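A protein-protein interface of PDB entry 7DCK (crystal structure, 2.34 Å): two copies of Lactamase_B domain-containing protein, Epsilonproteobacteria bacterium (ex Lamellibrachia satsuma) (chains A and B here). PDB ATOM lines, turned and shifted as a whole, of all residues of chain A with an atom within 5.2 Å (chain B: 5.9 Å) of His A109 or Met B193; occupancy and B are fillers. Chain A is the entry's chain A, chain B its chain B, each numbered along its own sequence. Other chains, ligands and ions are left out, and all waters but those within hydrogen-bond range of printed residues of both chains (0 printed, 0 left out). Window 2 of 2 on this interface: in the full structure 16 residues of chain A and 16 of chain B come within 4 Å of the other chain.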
ATOM      1  N   SER A 107      15.978   0.624 -14.160  1.00  0.00           N
ATOM      2  CA  SER A 107      16.409   1.223 -12.905  1.00  0.00           C
ATOM      3  C   SER A 107      17.394   2.355 -13.170  1.00  0.00           C
ATOM      4  O   SER A 107      18.312   2.226 -13.986  1.00  0.00           O
ATOM      5  CB  SER A 107      17.051   0.164 -12.010  1.00  0.00           C
ATOM      6  OG  SER A 107      17.824   0.761 -10.983  1.00  0.00           O
ATOM      7  N   LYS A 108      17.192   3.483 -12.486  1.00  0.00           N
ATOM      8  CA  LYS A 108      18.144   4.582 -12.614  1.00  0.00           C
ATOM      9  C   LYS A 108      19.511   4.186 -12.080  1.00  0.00           C
ATOM     10  O   LYS A 108      20.533   4.703 -12.545  1.00  0.00           O
ATOM     11  CB  LYS A 108      17.620   5.829 -11.903  1.00  0.00           C
ATOM     12  CG  LYS A 108      16.153   6.151 -12.226  1.00  0.00           C
ATOM     13  CD  LYS A 108      16.004   7.144 -13.388  1.00  0.00           C
ATOM     14  CE  LYS A 108      15.569   6.433 -14.680  1.00  0.00           C
ATOM     15  NZ  LYS A 108      15.695   7.281 -15.906  1.00  0.00           N
ATOM     16  N   HIS A 109      19.551   3.252 -11.129  1.00  0.00           N
ATOM     17  CA  HIS A 109      20.826   2.718 -10.667  1.00  0.00           C
ATOM     18  C   HIS A 109      21.538   1.959 -11.780  1.00  0.00           C
ATOM     19  O   HIS A 109      22.764   2.056 -11.923  1.00  0.00           O
ATOM     20  CB  HIS A 109      20.604   1.809  -9.462  1.00  0.00           C
ATOM     21  CG  HIS A 109      20.142   2.531  -8.236  1.00  0.00           C
ATOM     22  ND1 HIS A 109      20.956   3.387  -7.525  1.00  0.00           N
ATOM     23  CD2 HIS A 109      18.954   2.519  -7.587  1.00  0.00           C
ATOM     24  CE1 HIS A 109      20.290   3.872  -6.493  1.00  0.00           C
ATOM     25  NE2 HIS A 109      19.072   3.362  -6.509  1.00  0.00           N
ATOM     26  N   LEU A 110      20.784   1.190 -12.571  1.00  0.00           N
ATOM     27  CA  LEU A 110      21.382   0.464 -13.686  1.00  0.00           C
ATOM     28  C   LEU A 110      21.808   1.417 -14.797  1.00  0.00           C
ATOM     29  O   LEU A 110      22.862   1.225 -15.418  1.00  0.00           O
ATOM     30  CB  LEU A 110      20.401  -0.588 -14.212  1.00  0.00           C
ATOM     31  CG  LEU A 110      20.835  -1.411 -15.431  1.00  0.00           C
ATOM     32  CD1 LEU A 110      22.241  -1.986 -15.258  1.00  0.00           C
ATOM     33  CD2 LEU A 110      19.832  -2.518 -15.695  1.00  0.00           C
ATOM     34  N   ILE A 111      21.006   2.451 -15.062  1.00  0.00           N
ATOM     35  CA  ILE A 111      21.373   3.431 -16.080  1.00  0.00           C
ATOM     36  C   ILE A 111      22.643   4.168 -15.676  1.00  0.00           C
ATOM     37  O   ILE A 111      23.541   4.390 -16.498  1.00  0.00           O
ATOM     38  CB  ILE A 111      20.205   4.404 -16.330  1.00  0.00           C
ATOM     39  CG1 ILE A 111      19.057   3.683 -17.041  1.00  0.00           C
ATOM     40  CG2 ILE A 111      20.679   5.608 -17.140  1.00  0.00           C
ATOM     41  CD1 ILE A 111      17.712   4.375 -16.898  1.00  0.00           C
ATOM     42  N   ARG A 112      22.744   4.555 -14.403  1.00  0.00           N
ATOM     43  CA  ARG A 112      23.965   5.190 -13.915  1.00  0.00           C
ATOM     44  C   ARG A 112      25.183   4.304 -14.164  1.00  0.00           C
ATOM     45  O   ARG A 112      26.225   4.776 -14.639  1.00  0.00           O
ATOM     46  CB  ARG A 112      23.814   5.514 -12.428  1.00  0.00           C
ATOM     47  CG  ARG A 112      25.070   6.035 -11.752  1.00  0.00           C
ATOM     48  CD  ARG A 112      24.740   6.679 -10.402  1.00  0.00           C
ATOM     49  NE  ARG A 112      25.925   6.855  -9.562  1.00  0.00           N
ATOM     50  CZ  ARG A 112      26.730   7.915  -9.603  1.00  0.00           C
ATOM     51  NH1 ARG A 112      26.488   8.908 -10.451  1.00  0.00           N
ATOM     52  NH2 ARG A 112      27.783   7.985  -8.798  1.00  0.00           N
ATOM     53  N   ASP A 113      25.056   3.004 -13.877  1.00  0.00           N
ATOM     54  CA  ASP A 113      26.180   2.088 -14.044  1.00  0.00           C
ATOM     55  C   ASP A 113      26.551   1.923 -15.512  1.00  0.00           C
ATOM     56  O   ASP A 113      27.739   1.891 -15.857  1.00  0.00           O
ATOM     57  CB  ASP A 113      25.850   0.729 -13.425  1.00  0.00           C
ATOM     58  CG  ASP A 113      25.989   0.725 -11.905  1.00  0.00           C
ATOM     59  OD1 ASP A 113      26.468   1.737 -11.348  1.00  0.00           O
ATOM     60  OD2 ASP A 113      25.627  -0.292 -11.266  1.00  0.00           O
ATOM     61  N   TRP B  34      26.122  -1.219  -8.404  1.00  0.00           N
ATOM     62  CA  TRP B  34      24.880  -1.395  -7.660  1.00  0.00           C
ATOM     63  C   TRP B  34      24.531  -2.875  -7.562  1.00  0.00           C
ATOM     64  O   TRP B  34      24.315  -3.539  -8.584  1.00  0.00           O
ATOM     65  CB  TRP B  34      23.734  -0.626  -8.307  1.00  0.00           C
ATOM     66  CG  TRP B  34      22.578  -0.486  -7.375  1.00  0.00           C
ATOM     67  CD1 TRP B  34      21.425  -1.212  -7.379  1.00  0.00           C
ATOM     68  CD2 TRP B  34      22.477   0.424  -6.275  1.00  0.00           C
ATOM     69  NE1 TRP B  34      20.604  -0.802  -6.355  1.00  0.00           N
ATOM     70  CE2 TRP B  34      21.227   0.203  -5.663  1.00  0.00           C
ATOM     71  CE3 TRP B  34      23.319   1.412  -5.755  1.00  0.00           C
ATOM     72  CZ2 TRP B  34      20.799   0.931  -4.557  1.00  0.00           C
ATOM     73  CZ3 TRP B  34      22.892   2.135  -4.655  1.00  0.00           C
ATOM     74  CH2 TRP B  34      21.647   1.891  -4.068  1.00  0.00           C
ATOM     75  N   TRP B  82      17.457  -7.482 -10.694  1.00  0.00           N
ATOM     76  CA  TRP B  82      18.632  -7.482 -11.567  1.00  0.00           C
ATOM     77  C   TRP B  82      19.938  -7.378 -10.784  1.00  0.00           C
ATOM     78  O   TRP B  82      20.956  -7.950 -11.185  1.00  0.00           O
ATOM     79  CB  TRP B  82      18.528  -6.327 -12.575  1.00  0.00           C
ATOM     80  CG  TRP B  82      18.492  -4.977 -11.915  1.00  0.00           C
ATOM     81  CD1 TRP B  82      17.406  -4.375 -11.342  1.00  0.00           C
ATOM     82  CD2 TRP B  82      19.594  -4.071 -11.730  1.00  0.00           C
ATOM     83  NE1 TRP B  82      17.761  -3.152 -10.819  1.00  0.00           N
ATOM     84  CE2 TRP B  82      19.095  -2.941 -11.044  1.00  0.00           C
ATOM     85  CE3 TRP B  82      20.947  -4.103 -12.080  1.00  0.00           C
ATOM     86  CZ2 TRP B  82      19.905  -1.856 -10.702  1.00  0.00           C
ATOM     87  CZ3 TRP B  82      21.749  -3.021 -11.739  1.00  0.00           C
ATOM     88  CH2 TRP B  82      21.226  -1.918 -11.056  1.00  0.00           C
ATOM     89  N   PHE B 190      19.169  -2.867   3.534  1.00  0.00           N
ATOM     90  CA  PHE B 190      17.952  -2.672   4.313  1.00  0.00           C
ATOM     91  C   PHE B 190      16.864  -1.926   3.549  1.00  0.00           C
ATOM     92  O   PHE B 190      15.748  -1.803   4.062  1.00  0.00           O
ATOM     93  CB  PHE B 190      18.270  -1.926   5.617  1.00  0.00           C
ATOM     94  CG  PHE B 190      19.139  -2.704   6.577  1.00  0.00           C
ATOM     95  CD1 PHE B 190      19.470  -4.028   6.333  1.00  0.00           C
ATOM     96  CD2 PHE B 190      19.611  -2.109   7.737  1.00  0.00           C
ATOM     97  CE1 PHE B 190      20.267  -4.739   7.219  1.00  0.00           C
ATOM     98  CE2 PHE B 190      20.404  -2.816   8.629  1.00  0.00           C
ATOM     99  CZ  PHE B 190      20.736  -4.132   8.369  1.00  0.00           C
ATOM    100  N   HIS B 191      17.159  -1.439   2.341  1.00  0.00           N
ATOM    101  CA  HIS B 191      16.206  -0.691   1.512  1.00  0.00           C
ATOM    102  C   HIS B 191      15.548   0.444   2.292  1.00  0.00           C
ATOM    103  O   HIS B 191      14.325   0.596   2.301  1.00  0.00           O
ATOM    104  CB  HIS B 191      15.141  -1.608   0.908  1.00  0.00           C
ATOM    105  CG  HIS B 191      14.647  -1.158  -0.431  1.00  0.00           C
ATOM    106  ND1 HIS B 191      15.359  -1.357  -1.596  1.00  0.00           N
ATOM    107  CD2 HIS B 191      13.516  -0.504  -0.788  1.00  0.00           C
ATOM    108  CE1 HIS B 191      14.684  -0.846  -2.612  1.00  0.00           C
ATOM    109  NE2 HIS B 191      13.563  -0.323  -2.149  1.00  0.00           N
ATOM    110  N   LEU B 192      16.377   1.247   2.955  1.00  0.00           N
ATOM    111  CA  LEU B 192      15.914   2.439   3.652  1.00  0.00           C
ATOM    112  C   LEU B 192      16.340   3.720   2.946  1.00  0.00           C
ATOM    113  O   LEU B 192      16.183   4.809   3.509  1.00  0.00           O
ATOM    114  CB  LEU B 192      16.424   2.437   5.094  1.00  0.00           C
ATOM    115  CG  LEU B 192      15.968   1.253   5.946  1.00  0.00           C
ATOM    116  CD1 LEU B 192      16.836   1.119   7.186  1.00  0.00           C
ATOM    117  CD2 LEU B 192      14.506   1.415   6.328  1.00  0.00           C
ATOM    118  N   MET B 193      16.856   3.616   1.720  1.00  0.00           N
ATOM    119  CA  MET B 193      17.459   4.761   1.048  1.00  0.00           C
ATOM    120  C   MET B 193      16.443   5.829   0.665  1.00  0.00           C
ATOM    121  O   MET B 193      16.828   6.986   0.471  1.00  0.00           O
ATOM    122  CB  MET B 193      18.216   4.294  -0.197  1.00  0.00           C
ATOM    123  CG  MET B 193      17.346   3.578  -1.219  1.00  0.00           C
ATOM    124  SD  MET B 193      18.323   3.002  -2.619  1.00  0.00           S
ATOM    125  CE  MET B 193      19.392   4.418  -2.836  1.00  0.00           C
ATOM    126  N   TYR B 194      15.164   5.476   0.549  1.00  0.00           N
ATOM    127  CA  TYR B 194      14.128   6.433   0.189  1.00  0.00           C
ATOM    128  C   TYR B 194      13.325   6.914   1.392  1.00  0.00           C
ATOM    129  O   TYR B 194      12.331   7.624   1.213  1.00  0.00           O
ATOM    130  CB  TYR B 194      13.188   5.827  -0.859  1.00  0.00           C
ATOM    131  CG  TYR B 194      13.897   5.365  -2.113  1.00  0.00           C
ATOM    132  CD1 TYR B 194      14.596   6.263  -2.909  1.00  0.00           C
ATOM    133  CD2 TYR B 194      13.872   4.030  -2.499  1.00  0.00           C
ATOM    134  CE1 TYR B 194      15.250   5.844  -4.058  1.00  0.00           C
ATOM    135  CE2 TYR B 194      14.522   3.601  -3.643  1.00  0.00           C
ATOM    136  CZ  TYR B 194      15.210   4.513  -4.420  1.00  0.00           C
ATOM    137  OH  TYR B 194      15.859   4.092  -5.559  1.00  0.00           O
ATOM    138  N   GLU B 195      13.735   6.556   2.605  1.00  0.00           N
ATOM    139  CA  GLU B 195      12.996   6.886   3.815  1.00  0.00           C
ATOM    140  C   GLU B 195      13.564   8.138   4.472  1.00  0.00           C
ATOM    141  O   GLU B 195      14.756   8.436   4.362  1.00  0.00           O
ATOM    142  CB  GLU B 195      13.028   5.722   4.809  1.00  0.00           C
ATOM    143  CG  GLU B 195      12.691   4.375   4.195  1.00  0.00           C
ATOM    144  CD  GLU B 195      11.229   4.265   3.816  1.00  0.00           C
ATOM    145  OE1 GLU B 195      10.371   4.618   4.651  1.00  0.00           O
ATOM    146  OE2 GLU B 195      10.935   3.828   2.681  1.00  0.00           O
ATOM    147  N   CYS B 220      21.638  -1.201  -0.477  1.00  0.00           N
ATOM    148  CA  CYS B 220      20.555  -0.260  -0.722  1.00  0.00           C
ATOM    149  C   CYS B 220      20.061   0.404   0.549  1.00  0.00           C
ATOM    150  O   CYS B 220      18.972   0.989   0.552  1.00  0.00           O
ATOM    151  CB  CYS B 220      19.399  -0.955  -1.447  1.00  0.00           C
ATOM    152  SG  CYS B 220      18.629  -2.384  -0.618  1.00  0.00           S
ATOM    153  N   SER B 221      20.855   0.346   1.617  1.00  0.00           N
ATOM    154  CA  SER B 221      20.410   0.836   2.916  1.00  0.00           C
ATOM    155  C   SER B 221      20.215   2.348   2.935  1.00  0.00           C
ATOM    156  O   SER B 221      19.322   2.847   3.629  1.00  0.00           O
ATOM    157  CB  SER B 221      21.411   0.428   3.996  1.00  0.00           C
ATOM    158  OG  SER B 221      21.283  -0.948   4.306  1.00  0.00           O
ATOM    159  N   GLY B 222      21.042   3.092   2.206  1.00  0.00           N
ATOM    160  CA  GLY B 222      20.928   4.538   2.182  1.00  0.00           C
ATOM    161  C   GLY B 222      21.950   5.256   3.042  1.00  0.00           C
ATOM    162  O   GLY B 222      22.238   4.821   4.160  1.00  0.00           O
ATOM    163  N   ASP B 223      22.498   6.366   2.533  1.00  0.00           N
ATOM    164  CA  ASP B 223      23.511   7.105   3.283  1.00  0.00           C
ATOM    165  C   ASP B 223      22.949   7.658   4.585  1.00  0.00           C
ATOM    166  O   ASP B 223      23.634   7.654   5.616  1.00  0.00           O
ATOM    167  CB  ASP B 223      24.081   8.236   2.431  1.00  0.00           C
ATOM    168  CG  ASP B 223      24.889   7.729   1.256  1.00  0.00           C
ATOM    169  OD1 ASP B 223      25.585   6.704   1.416  1.00  0.00           O
ATOM    170  OD2 ASP B 223      24.833   8.359   0.177  1.00  0.00           O
ATOM    171  N   ALA B 225      20.308   6.477   6.464  1.00  0.00           N
ATOM    172  CA  ALA B 225      20.096   5.383   7.407  1.00  0.00           C
ATOM    173  C   ALA B 225      21.415   4.871   7.975  1.00  0.00           C
ATOM    174  O   ALA B 225      21.524   4.624   9.181  1.00  0.00           O
ATOM    175  CB  ALA B 225      19.326   4.250   6.726  1.00  0.00           C
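The side-chain hydroxyl (OH) of Tyr B194 sits at hydrogen-bond distance from a ring nitrogen (NE2) of His A109. The side-chain carboxylate of Asp A113 is in hydrogen-bond range of the backbone NH of Trp B34, 3.0 Å away.
OG of Ser A107 sits at hydrogen-bond distance from N of His A109 (3.0 Å). The side-chain hydroxyl of Ser A107 is in hydrogen-bond range of the backbone NH of Leu A110 (3.4 Å). N of Met B193 sits at hydrogen-bond distance from O of Ser B221 (3.2 Å).
OG of Ser A107 touches CZ2 of Trp B82 (3.4 Å). CE1 of His A109 touches CH2 of Trp B34, 3.4 Å away. CB of His A109 touches CZ2 of Trp B82 (3.9 Å). His A109 touches Met B193 (CE1 to CE, 3.8 Å). Leu A110 touches Trp B82.
Printed residues of chain B within 4 Å of Ser A107: Trp B82 (3.4 Å). Of the printed residues of chain B, Leu A110 touches Trp B82 (3.5 Å). Of the printed residues of chain A, Trp B34 touches His A109 and Asp A113. Of chain A, only His A109 (3.8 Å) comes within 4 Å of Met B193. The nearest printed residue of chain B that does not touch His A109 is Cys B220 (6.7 Å).
Printed residues of chain B that touch a printed residue of chain A: Trp B34, Trp B82, Met B193 and Tyr B194. Printed residues of chain A that touch a printed residue of chain B: Ser A107, His A109, Leu A110 and Asp A113.
No position is printed for both chains. Of the 7 pairs that touch across the chains among the printed residues, none has its exchanged pair printed and touching as well.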
